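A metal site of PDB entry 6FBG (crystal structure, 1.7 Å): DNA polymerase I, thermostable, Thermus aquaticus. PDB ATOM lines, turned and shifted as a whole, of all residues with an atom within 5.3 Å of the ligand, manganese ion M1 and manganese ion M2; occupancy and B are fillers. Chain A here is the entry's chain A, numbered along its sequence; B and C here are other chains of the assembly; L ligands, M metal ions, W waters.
A nitrogen (N2) of the ligand sits close to N3 of DG 5 of chain C (3.2 Å).
O2 of DC 4 of chain C is in hydrogen-bond range of N2 of the ligand (2.7 Å).
An oxygen (O4) of the ligand lies within hydrogen-bond range of the backbone NH of Gln 322 (3.1 Å).
NH1 of Arg 368 lies within salt-bridge range of O7 of the ligand (2.7 Å).
The guanidinium group (NH2) of Arg 282 lies within hydrogen-bond range of an oxygen (O11) of the ligand, at 3.3 Å.
NE2 of His 348 is in hydrogen-bond range of O6 of the ligand (3.0 Å).
N of Glu 324 lies within hydrogen-bond range of O8 of the ligand, at 3.2 Å.
N of Ile 323 sits close to O3 of the ligand (3.2 Å).
The side-chain amino group of Lys 372 sits at hydrogen-bond distance from a nitrogen (N4) of the ligand (2.9 Å).
NE2 of Gln 322 sits at hydrogen-bond distance from OG of Ser 321, at 3.3 Å.
OP2 of DC 12 of chain B is in salt-bridge range of NH1 of Arg 369 (2.5 Å).
The side-chain carboxylate (OE1) of Glu 324 is in hydrogen-bond range of the side-chain hydroxyl (OH) of Tyr 380 (2.7 Å).
O2 of DC 12 of chain B lies close to N2 of DG 5 of chain C (2.7 Å).
O2 of DC 12 of chain B sits at hydrogen-bond distance from NH1 of Arg 282, at 2.8 Å.
Ser 321 touches the ligand.
CZ of Phe 376 touches O8 of the ligand, 3.1 Å away.
Tyr 380 touches the ligand.
Hydrophobic or aromatic side chains that line the ligand: Ile 323, His 348, Phe 376 and Tyr 380.
Of the 23 residues printed, 16 come within 4 Å of the ligand.
The nearest printed residue that does not touch the ligand is Thr 373 (4.2 Å).
Within 4 Å of manganese ion M1: Asp 319, Tyr 320 and Asp 494.
Three residues have an atom within 4 Å of manganese ion M2: Asp 319, Asp 494 and DC 12 of chain B.
The nearest printed residue that does not touch manganese ion M2 is Glu 495 (4.2 Å).
Manganese ion M1 is bound by O10 of the ligand, O of Tyr 320, OD1 of Asp 319, OD2 of Asp 494, O3 of the ligand and O2 of the ligand.
OD1 of Asp 494 binds manganese ion M2 (2.1 Å).
Manganese ion M2 is bound by OD2 of Asp 319, 2.2 Å away.
Manganese ion M2 is bound by water W2 (2.2 Å).
O2 of the ligand is bound to manganese ion M2 (2.2 Å).
Water W4 is bound to manganese ion M2, 2.2 Å away.
Manganese ion M2 is bound by O3' of DC 12 of chain B, 2.2 Å away.
Manganese ion M2 has six donor atoms within binding distance.
Water W2 bridges OE1 of Glu 495 and O of Val 492.
Water W4 lies within hydrogen-bond range of an oxygen (O5) of the ligand and OP1 of DC 12 of chain B.
Water W7 lies within hydrogen-bond range of an oxygen (O1) of the ligand (2.6 Å), the side-chain hydroxyl (OG1) of Thr 373 (2.8 Å), the side-chain amino group (NZ) of Lys 372 (2.9 Å) and N4 of DC 12 of chain B (3.2 Å).
Water W6 bridges the backbone carbonyl oxygen (O) of Asp 319 (2.8 Å) and an oxygen (O4) of the ligand (3.5 Å).
Water W5 lies within hydrogen-bond range of OP2 of DC 12 of chain B, NZ of Lys 372, O5 of the ligand and NH2 of Arg 369.
Water W3 lies within hydrogen-bond range of OE2 of Glu 324, NH2 of Arg 282 and O11 of the ligand.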
ATOM      1  N   ARG A 282     -24.209  15.331   8.599  1.00  0.00           N
ATOM      2  CA  ARG A 282     -22.874  15.857   8.362  1.00  0.00           C
ATOM      3  C   ARG A 282     -22.952  17.234   7.710  1.00  0.00           C
ATOM      4  O   ARG A 282     -23.907  17.554   7.005  1.00  0.00           O
ATOM      5  CB  ARG A 282     -22.070  14.924   7.462  1.00  0.00           C
ATOM      6  CG  ARG A 282     -21.368  13.776   8.145  1.00  0.00           C
ATOM      7  CD  ARG A 282     -20.435  13.109   7.147  1.00  0.00           C
ATOM      8  NE  ARG A 282     -19.544  12.128   7.747  1.00  0.00           N
ATOM      9  CZ  ARG A 282     -18.561  11.530   7.083  1.00  0.00           C
ATOM     10  NH1 ARG A 282     -18.353  11.798   5.810  1.00  0.00           N
ATOM     11  NH2 ARG A 282     -17.788  10.649   7.705  1.00  0.00           N
ATOM     12  N   ASP A 319      -8.667  15.015  16.197  1.00  0.00           N
ATOM     13  CA  ASP A 319      -9.405  14.021  15.418  1.00  0.00           C
ATOM     14  C   ASP A 319      -9.873  12.904  16.342  1.00  0.00           C
ATOM     15  O   ASP A 319      -9.047  12.274  17.015  1.00  0.00           O
ATOM     16  CB  ASP A 319      -8.536  13.474  14.293  1.00  0.00           C
ATOM     17  CG  ASP A 319      -9.282  12.535  13.381  1.00  0.00           C
ATOM     18  OD1 ASP A 319      -9.762  11.497  13.874  1.00  0.00           O
ATOM     19  OD2 ASP A 319      -9.399  12.842  12.182  1.00  0.00           O
ATOM     20  N   TYR A 320     -11.179  12.653  16.363  1.00  0.00           N
ATOM     21  CA  TYR A 320     -11.724  11.586  17.198  1.00  0.00           C
ATOM     22  C   TYR A 320     -11.186  10.227  16.747  1.00  0.00           C
ATOM     23  O   TYR A 320     -11.127   9.934  15.555  1.00  0.00           O
ATOM     24  CB  TYR A 320     -13.257  11.577  17.134  1.00  0.00           C
ATOM     25  CG  TYR A 320     -13.953  12.636  17.959  1.00  0.00           C
ATOM     26  CD1 TYR A 320     -14.079  12.507  19.342  1.00  0.00           C
ATOM     27  CD2 TYR A 320     -14.512  13.756  17.361  1.00  0.00           C
ATOM     28  CE1 TYR A 320     -14.730  13.470  20.098  1.00  0.00           C
ATOM     29  CE2 TYR A 320     -15.153  14.725  18.111  1.00  0.00           C
ATOM     30  CZ  TYR A 320     -15.263  14.580  19.475  1.00  0.00           C
ATOM     31  OH  TYR A 320     -15.905  15.544  20.217  1.00  0.00           O
ATOM     32  N   SER A 321     -10.805   9.412  17.722  1.00  0.00           N
ATOM     33  CA  SER A 321     -10.301   8.067  17.454  1.00  0.00           C
ATOM     34  C   SER A 321     -11.450   7.110  17.140  1.00  0.00           C
ATOM     35  O   SER A 321     -12.408   7.009  17.912  1.00  0.00           O
ATOM     36  CB  SER A 321      -9.500   7.558  18.654  1.00  0.00           C
ATOM     37  OG  SER A 321      -9.295   6.158  18.578  1.00  0.00           O
ATOM     38  N   GLN A 322     -11.340   6.407  16.016  1.00  0.00           N
ATOM     39  CA  GLN A 322     -12.249   5.299  15.674  1.00  0.00           C
ATOM     40  C   GLN A 322     -13.697   5.665  15.964  1.00  0.00           C
ATOM     41  O   GLN A 322     -14.439   4.913  16.596  1.00  0.00           O
ATOM     42  CB  GLN A 322     -11.854   4.041  16.454  1.00  0.00           C
ATOM     43  CG  GLN A 322     -10.371   3.732  16.461  1.00  0.00           C
ATOM     44  CD  GLN A 322     -10.052   2.553  17.365  1.00  0.00           C
ATOM     45  OE1 GLN A 322     -10.293   1.396  17.009  1.00  0.00           O
ATOM     46  NE2 GLN A 322      -9.505   2.837  18.544  1.00  0.00           N
ATOM     47  N   ILE A 323     -14.123   6.835  15.471  1.00  0.00           N
ATOM     48  CA  ILE A 323     -15.285   7.485  16.056  1.00  0.00           C
ATOM     49  C   ILE A 323     -16.550   6.672  15.807  1.00  0.00           C
ATOM     50  O   ILE A 323     -17.328   6.410  16.732  1.00  0.00           O
ATOM     51  CB  ILE A 323     -15.419   8.931  15.555  1.00  0.00           C
ATOM     52  CG1 ILE A 323     -16.617   9.620  16.220  1.00  0.00           C
ATOM     53  CG2 ILE A 323     -15.544   8.999  14.039  1.00  0.00           C
ATOM     54  CD1 ILE A 323     -16.536   9.665  17.743  1.00  0.00           C
ATOM     55  N   GLU A 324     -16.794   6.249  14.565  1.00  0.00           N
ATOM     56  CA  GLU A 324     -18.060   5.566  14.290  1.00  0.00           C
ATOM     57  C   GLU A 324     -18.108   4.179  14.929  1.00  0.00           C
ATOM     58  O   GLU A 324     -19.195   3.684  15.223  1.00  0.00           O
ATOM     59  CB  GLU A 324     -18.313   5.488  12.780  1.00  0.00           C
ATOM     60  CG  GLU A 324     -18.958   6.787  12.253  1.00  0.00           C
ATOM     61  CD  GLU A 324     -19.391   6.716  10.793  1.00  0.00           C
ATOM     62  OE1 GLU A 324     -19.702   5.607  10.311  1.00  0.00           O
ATOM     63  OE2 GLU A 324     -19.402   7.775  10.131  1.00  0.00           O
ATOM     64  N   LEU A 325     -16.949   3.560  15.185  1.00  0.00           N
ATOM     65  CA  LEU A 325     -16.954   2.317  15.950  1.00  0.00           C
ATOM     66  C   LEU A 325     -17.302   2.570  17.409  1.00  0.00           C
ATOM     67  O   LEU A 325     -18.061   1.799  18.009  1.00  0.00           O
ATOM     68  CB  LEU A 325     -15.592   1.623  15.840  1.00  0.00           C
ATOM     69  CG  LEU A 325     -15.215   1.130  14.437  1.00  0.00           C
ATOM     70  CD1 LEU A 325     -13.809   0.548  14.426  1.00  0.00           C
ATOM     71  CD2 LEU A 325     -16.218   0.113  13.921  1.00  0.00           C
ATOM     72  N   HIS A 348      -8.542  -0.593  14.069  1.00  0.00           N
ATOM     73  CA  HIS A 348      -7.896  -0.345  12.780  1.00  0.00           C
ATOM     74  C   HIS A 348      -6.502  -0.973  12.753  1.00  0.00           C
ATOM     75  O   HIS A 348      -6.140  -1.666  11.796  1.00  0.00           O
ATOM     76  CB  HIS A 348      -7.816   1.148  12.504  1.00  0.00           C
ATOM     77  CG  HIS A 348      -9.148   1.799  12.317  1.00  0.00           C
ATOM     78  ND1 HIS A 348     -10.263   1.102  11.906  1.00  0.00           N
ATOM     79  CD2 HIS A 348      -9.550   3.085  12.478  1.00  0.00           C
ATOM     80  CE1 HIS A 348     -11.298   1.924  11.828  1.00  0.00           C
ATOM     81  NE2 HIS A 348     -10.890   3.137  12.168  1.00  0.00           N
ATOM     82  N   ARG A 368      -2.656   1.170   8.293  1.00  0.00           N
ATOM     83  CA  ARG A 368      -3.792   1.405   9.175  1.00  0.00           C
ATOM     84  C   ARG A 368      -4.945   2.073   8.418  1.00  0.00           C
ATOM     85  O   ARG A 368      -6.115   1.762   8.669  1.00  0.00           O
ATOM     86  CB  ARG A 368      -3.367   2.257  10.369  1.00  0.00           C
ATOM     87  CG  ARG A 368      -4.431   2.398  11.433  1.00  0.00           C
ATOM     88  CD  ARG A 368      -3.904   3.096  12.681  1.00  0.00           C
ATOM     89  NE  ARG A 368      -4.950   3.242  13.688  1.00  0.00           N
ATOM     90  CZ  ARG A 368      -5.875   4.203  13.675  1.00  0.00           C
ATOM     91  NH1 ARG A 368      -5.885   5.102  12.704  1.00  0.00           N
ATOM     92  NH2 ARG A 368      -6.793   4.252  14.632  1.00  0.00           N
ATOM     93  N   ARG A 369      -4.618   2.987   7.504  1.00  0.00           N
ATOM     94  CA  ARG A 369      -5.652   3.614   6.686  1.00  0.00           C
ATOM     95  C   ARG A 369      -6.392   2.588   5.844  1.00  0.00           C
ATOM     96  O   ARG A 369      -7.619   2.619   5.742  1.00  0.00           O
ATOM     97  CB  ARG A 369      -5.024   4.697   5.808  1.00  0.00           C
ATOM     98  CG  ARG A 369      -5.900   5.137   4.649  1.00  0.00           C
ATOM     99  CD  ARG A 369      -5.364   6.408   4.010  1.00  0.00           C
ATOM    100  NE  ARG A 369      -5.466   7.554   4.921  1.00  0.00           N
ATOM    101  CZ  ARG A 369      -6.566   8.293   5.074  1.00  0.00           C
ATOM    102  NH1 ARG A 369      -6.561   9.303   5.927  1.00  0.00           N
ATOM    103  NH2 ARG A 369      -7.661   8.025   4.381  1.00  0.00           N
ATOM    104  N   LYS A 372      -8.780   0.769   8.048  1.00  0.00           N
ATOM    105  CA  LYS A 372      -9.970   1.570   8.315  1.00  0.00           C
ATOM    106  C   LYS A 372     -11.023   1.338   7.232  1.00  0.00           C
ATOM    107  O   LYS A 372     -12.205   1.131   7.538  1.00  0.00           O
ATOM    108  CB  LYS A 372      -9.580   3.050   8.381  1.00  0.00           C
ATOM    109  CG  LYS A 372     -10.758   4.019   8.557  1.00  0.00           C
ATOM    110  CD  LYS A 372     -10.584   5.268   7.687  1.00  0.00           C
ATOM    111  CE  LYS A 372     -10.789   4.951   6.204  1.00  0.00           C
ATOM    112  NZ  LYS A 372     -10.955   6.187   5.385  1.00  0.00           N
ATOM    113  N   THR A 373     -10.612   1.374   5.968  1.00  0.00           N
ATOM    114  CA  THR A 373     -11.548   1.160   4.871  1.00  0.00           C
ATOM    115  C   THR A 373     -12.191  -0.219   4.968  1.00  0.00           C
ATOM    116  O   THR A 373     -13.398  -0.369   4.739  1.00  0.00           O
ATOM    117  CB  THR A 373     -10.820   1.336   3.537  1.00  0.00           C
ATOM    118  OG1 THR A 373     -10.205   2.624   3.496  1.00  0.00           O
ATOM    119  CG2 THR A 373     -11.783   1.200   2.368  1.00  0.00           C
ATOM    120  N   PHE A 376     -14.863  -0.414   8.110  1.00  0.00           N
ATOM    121  CA  PHE A 376     -16.153   0.213   7.868  1.00  0.00           C
ATOM    122  C   PHE A 376     -16.842  -0.349   6.627  1.00  0.00           C
ATOM    123  O   PHE A 376     -18.071  -0.432   6.590  1.00  0.00           O
ATOM    124  CB  PHE A 376     -15.986   1.726   7.730  1.00  0.00           C
ATOM    125  CG  PHE A 376     -15.571   2.381   9.010  1.00  0.00           C
ATOM    126  CD1 PHE A 376     -16.412   2.364  10.103  1.00  0.00           C
ATOM    127  CD2 PHE A 376     -14.341   3.004   9.124  1.00  0.00           C
ATOM    128  CE1 PHE A 376     -16.040   2.949  11.292  1.00  0.00           C
ATOM    129  CE2 PHE A 376     -13.954   3.609  10.309  1.00  0.00           C
ATOM    130  CZ  PHE A 376     -14.811   3.575  11.392  1.00  0.00           C
ATOM    131  N   GLY A 377     -16.076  -0.757   5.616  1.00  0.00           N
ATOM    132  CA  GLY A 377     -16.682  -1.434   4.482  1.00  0.00           C
ATOM    133  C   GLY A 377     -17.454  -2.673   4.896  1.00  0.00           C
ATOM    134  O   GLY A 377     -18.602  -2.868   4.499  1.00  0.00           O
ATOM    135  N   TYR A 380     -20.718  -1.845   7.021  1.00  0.00           N
ATOM    136  CA  TYR A 380     -21.848  -1.306   6.297  1.00  0.00           C
ATOM    137  C   TYR A 380     -22.183  -2.104   5.046  1.00  0.00           C
ATOM    138  O   TYR A 380     -22.858  -1.591   4.146  1.00  0.00           O
ATOM    139  CB  TYR A 380     -21.590   0.174   5.963  1.00  0.00           C
ATOM    140  CG  TYR A 380     -21.429   1.025   7.208  1.00  0.00           C
ATOM    141  CD1 TYR A 380     -22.463   1.115   8.139  1.00  0.00           C
ATOM    142  CD2 TYR A 380     -20.263   1.730   7.453  1.00  0.00           C
ATOM    143  CE1 TYR A 380     -22.331   1.880   9.275  1.00  0.00           C
ATOM    144  CE2 TYR A 380     -20.128   2.501   8.597  1.00  0.00           C
ATOM    145  CZ  TYR A 380     -21.168   2.575   9.504  1.00  0.00           C
ATOM    146  OH  TYR A 380     -21.045   3.343  10.641  1.00  0.00           O
ATOM    147  N   ASN A 459     -26.631   2.878   8.383  1.00  0.00           N
ATOM    148  CA  ASN A 459     -25.451   3.736   8.462  1.00  0.00           C
ATOM    149  C   ASN A 459     -25.783   5.087   9.079  1.00  0.00           C
ATOM    150  O   ASN A 459     -24.975   5.644   9.840  1.00  0.00           O
ATOM    151  CB  ASN A 459     -24.858   3.928   7.063  1.00  0.00           C
ATOM    152  CG  ASN A 459     -23.795   5.020   7.023  1.00  0.00           C
ATOM    153  OD1 ASN A 459     -24.094   6.195   6.830  1.00  0.00           O
ATOM    154  ND2 ASN A 459     -22.535   4.624   7.216  1.00  0.00           N
ATOM    155  N   VAL A 492     -13.486  18.712   9.529  1.00  0.00           N
ATOM    156  CA  VAL A 492     -13.423  17.639   8.554  1.00  0.00           C
ATOM    157  C   VAL A 492     -14.145  16.424   9.137  1.00  0.00           C
ATOM    158  O   VAL A 492     -13.553  15.356   9.312  1.00  0.00           O
ATOM    159  CB  VAL A 492     -11.969  17.325   8.166  1.00  0.00           C
ATOM    160  CG1 VAL A 492     -11.909  16.398   6.959  1.00  0.00           C
ATOM    161  CG2 VAL A 492     -11.207  18.624   7.849  1.00  0.00           C
ATOM    162  N   ASP A 494     -14.922  14.568  11.639  1.00  0.00           N
ATOM    163  CA  ASP A 494     -14.585  14.220  13.011  1.00  0.00           C
ATOM    164  C   ASP A 494     -13.284  14.873  13.444  1.00  0.00           C
ATOM    165  O   ASP A 494     -12.635  14.410  14.391  1.00  0.00           O
ATOM    166  CB  ASP A 494     -14.514  12.697  13.197  1.00  0.00           C
ATOM    167  CG  ASP A 494     -13.180  12.122  12.744  1.00  0.00           C
ATOM    168  OD1 ASP A 494     -12.572  12.666  11.804  1.00  0.00           O
ATOM    169  OD2 ASP A 494     -12.750  11.110  13.337  1.00  0.00           O
ATOM    170  N   GLU A 495     -12.890  15.952  12.760  1.00  0.00           N
ATOM    171  CA  GLU A 495     -11.630  16.621  12.997  1.00  0.00           C
ATOM    172  C   GLU A 495     -11.839  18.119  12.982  1.00  0.00           C
ATOM    173  O   GLU A 495     -12.650  18.631  12.201  1.00  0.00           O
ATOM    174  CB  GLU A 495     -10.588  16.220  11.929  1.00  0.00           C
ATOM    175  CG  GLU A 495      -9.357  17.120  11.856  1.00  0.00           C
ATOM    176  CD  GLU A 495      -8.437  16.749  10.711  1.00  0.00           C
ATOM    177  OE1 GLU A 495      -8.810  15.867   9.906  1.00  0.00           O
ATOM    178  OE2 GLU A 495      -7.343  17.339  10.622  1.00  0.00           O
ATOM    179  P    DC B  12      -8.879  12.008   5.398  1.00  0.00           P
ATOM    180  OP1  DC B  12      -8.085  12.731   6.420  1.00  0.00           O
ATOM    181  OP2  DC B  12      -8.471  10.669   4.939  1.00  0.00           O
ATOM    182  O5'  DC B  12     -10.388  11.920   5.922  1.00  0.00           O
ATOM    183  C5'  DC B  12     -11.019  13.065   6.503  1.00  0.00           C
ATOM    184  C4'  DC B  12     -12.436  12.751   6.911  1.00  0.00           C
ATOM    185  O4'  DC B  12     -13.206  12.390   5.738  1.00  0.00           O
ATOM    186  C3'  DC B  12     -12.588  11.566   7.856  1.00  0.00           C
ATOM    187  O3'  DC B  12     -12.471  11.988   9.203  1.00  0.00           O
ATOM    188  C2'  DC B  12     -13.969  11.026   7.525  1.00  0.00           C
ATOM    189  C1'  DC B  12     -14.194  11.434   6.074  1.00  0.00           C
ATOM    190  N1   DC B  12     -14.095  10.293   5.100  1.00  0.00           N
ATOM    191  C2   DC B  12     -15.239   9.587   4.738  1.00  0.00           C
ATOM    192  O2   DC B  12     -16.330   9.915   5.240  1.00  0.00           O
ATOM    193  N3   DC B  12     -15.126   8.568   3.851  1.00  0.00           N
ATOM    194  C4   DC B  12     -13.938   8.262   3.336  1.00  0.00           C
ATOM    195  N4   DC B  12     -13.876   7.238   2.463  1.00  0.00           N
ATOM    196  C5   DC B  12     -12.754   8.966   3.689  1.00  0.00           C
ATOM    197  C6   DC B  12     -12.882   9.969   4.567  1.00  0.00           C
ATOM    198  P    DC C   4     -20.142  -3.762  -2.351  1.00  0.00           P
ATOM    199  OP1  DC C   4     -19.411  -3.016  -3.394  1.00  0.00           O
ATOM    200  OP2  DC C   4     -19.824  -5.181  -2.095  1.00  0.00           O
ATOM    201  O5'  DC C   4     -20.004  -2.956  -0.985  1.00  0.00           O
ATOM    202  C5'  DC C   4     -20.503  -1.626  -0.892  1.00  0.00           C
ATOM    203  C4'  DC C   4     -20.907  -1.292   0.526  1.00  0.00           C
ATOM    204  O4'  DC C   4     -19.761  -1.425   1.403  1.00  0.00           O
ATOM    205  C3'  DC C   4     -21.407   0.130   0.729  1.00  0.00           C
ATOM    206  O3'  DC C   4     -22.814   0.223   0.492  1.00  0.00           O
ATOM    207  C2'  DC C   4     -21.038   0.412   2.172  1.00  0.00           C
ATOM    208  C1'  DC C   4     -19.738  -0.368   2.343  1.00  0.00           C
ATOM    209  N1   DC C   4     -18.509   0.443   2.111  1.00  0.00           N
ATOM    210  C2   DC C   4     -18.145   1.424   3.035  1.00  0.00           C
ATOM    211  O2   DC C   4     -18.854   1.596   4.043  1.00  0.00           O
ATOM    212  N3   DC C   4     -17.026   2.156   2.819  1.00  0.00           N
ATOM    213  C4   DC C   4     -16.290   1.947   1.731  1.00  0.00           C
ATOM    214  N4   DC C   4     -15.198   2.686   1.554  1.00  0.00           N
ATOM    215  C5   DC C   4     -16.641   0.947   0.767  1.00  0.00           C
ATOM    216  C6   DC C   4     -17.754   0.234   0.993  1.00  0.00           C
ATOM    217  P    DG C   5     -23.433   1.462  -0.320  1.00  0.00           P
ATOM    218  OP1  DG C   5     -24.829   1.121  -0.672  1.00  0.00           O
ATOM    219  OP2  DG C   5     -22.461   1.839  -1.380  1.00  0.00           O
ATOM    220  O5'  DG C   5     -23.452   2.647   0.753  1.00  0.00           O
ATOM    221  C5'  DG C   5     -24.280   2.535   1.908  1.00  0.00           C
ATOM    222  C4'  DG C   5     -23.931   3.588   2.946  1.00  0.00           C
ATOM    223  O4'  DG C   5     -22.569   3.372   3.399  1.00  0.00           O
ATOM    224  C3'  DG C   5     -23.954   5.020   2.454  1.00  0.00           C
ATOM    225  O3'  DG C   5     -25.285   5.560   2.513  1.00  0.00           O
ATOM    226  C2'  DG C   5     -22.997   5.713   3.409  1.00  0.00           C
ATOM    227  C1'  DG C   5     -21.976   4.619   3.746  1.00  0.00           C
ATOM    228  N9   DG C   5     -20.717   4.763   3.010  1.00  0.00           N
ATOM    229  C8   DG C   5     -20.305   4.021   1.927  1.00  0.00           C
ATOM    230  N7   DG C   5     -19.119   4.368   1.488  1.00  0.00           N
ATOM    231  C5   DG C   5     -18.737   5.403   2.335  1.00  0.00           C
ATOM    232  C6   DG C   5     -17.550   6.180   2.356  1.00  0.00           C
ATOM    233  O6   DG C   5     -16.571   6.110   1.595  1.00  0.00           O
ATOM    234  N1   DG C   5     -17.569   7.121   3.385  1.00  0.00           N
ATOM    235  C2   DG C   5     -18.597   7.291   4.273  1.00  0.00           C
ATOM    236  N2   DG C   5     -18.443   8.251   5.199  1.00  0.00           N
ATOM    237  N3   DG C   5     -19.717   6.576   4.268  1.00  0.00           N
ATOM    238  C4   DG C   5     -19.711   5.653   3.280  1.00  0.00           C
HETATM  239  N1  LIG L   1     -16.342   4.077   4.755  1.00  0.00           N
HETATM  240  C1  LIG L   1     -17.332   4.457   5.616  1.00  0.00           C
HETATM  241  N2  LIG L   1     -18.518   3.846   5.495  1.00  0.00           N
HETATM  242  N3  LIG L   1     -17.175   5.385   6.550  1.00  0.00           N
HETATM  243  C2  LIG L   1     -15.933   5.923   6.548  1.00  0.00           C
HETATM  244  C3  LIG L   1     -14.882   5.620   5.706  1.00  0.00           C
HETATM  245  C4  LIG L   1     -15.073   4.608   4.714  1.00  0.00           C
HETATM  246  O1  LIG L   1     -14.241   4.198   3.910  1.00  0.00           O
HETATM  247  N4  LIG L   1     -13.774   6.402   6.025  1.00  0.00           N
HETATM  248  C5  LIG L   1     -14.166   7.121   7.046  1.00  0.00           C
HETATM  249  N5  LIG L   1     -15.467   6.873   7.420  1.00  0.00           N
HETATM  250  P1  LIG L   1     -11.353   8.916  10.176  1.00  0.00           P
HETATM  251  P2  LIG L   1     -11.469   6.907  12.343  1.00  0.00           P
HETATM  252  P3  LIG L   1      -8.843   7.217  13.545  1.00  0.00           P
HETATM  253  C6  LIG L   1     -16.178   7.370   8.603  1.00  0.00           C
HETATM  254  O2  LIG L   1     -11.027  10.000  11.076  1.00  0.00           O
HETATM  255  O3  LIG L   1     -12.139   7.914  13.136  1.00  0.00           O
HETATM  256  O4  LIG L   1      -8.456   6.697  14.898  1.00  0.00           O
HETATM  257  C7  LIG L   1     -16.082   6.420   9.786  1.00  0.00           C
HETATM  258  O5  LIG L   1     -10.430   9.025   8.903  1.00  0.00           O
HETATM  259  O6  LIG L   1     -12.426   5.665  12.201  1.00  0.00           O
HETATM  260  O7  LIG L   1      -7.753   7.051  12.504  1.00  0.00           O
HETATM  261  C8  LIG L   1     -14.908   6.991  10.575  1.00  0.00           C
HETATM  262  O8  LIG L   1     -15.012   6.648  11.961  1.00  0.00           O
HETATM  263  N6  LIG L   1     -11.099   7.446  10.848  1.00  0.00           N
HETATM  264  O9  LIG L   1     -10.108   6.404  13.002  1.00  0.00           O
HETATM  265  O10 LIG L   1      -9.273   8.683  13.567  1.00  0.00           O
HETATM  266  C9  LIG L   1     -15.112   8.485  10.365  1.00  0.00           C
HETATM  267  O11 LIG L   1     -15.577   8.599   8.997  1.00  0.00           O
HETATM  268  C10 LIG L   1     -13.891   9.347  10.566  1.00  0.00           C
HETATM  269  O12 LIG L   1     -12.842   8.921   9.674  1.00  0.00           O
HETATM  270 MN    MN M   1     -11.025   9.843  13.442  1.00  0.00          MN
HETATM  271 MN    MN M   2     -10.820  12.181  10.700  1.00  0.00          MN
HETATM  272  O   HOH W   1     -20.081   6.201   7.555  1.00  0.00           O
HETATM  273  O   HOH W   2     -10.574  14.054   9.626  1.00  0.00           O
HETATM  274  O   HOH W   3     -18.142  10.155  10.688  1.00  0.00           O
HETATM  275  O   HOH W   4      -9.254  11.545   9.250  1.00  0.00           O
HETATM  276  O   HOH W   5      -9.859   8.643   6.126  1.00  0.00           O
HETATM  277  O   HOH W   6      -8.001  10.065  15.580  1.00  0.00           O
HETATM  278  O   HOH W   7     -11.819   4.807   3.029  1.00  0.00           O
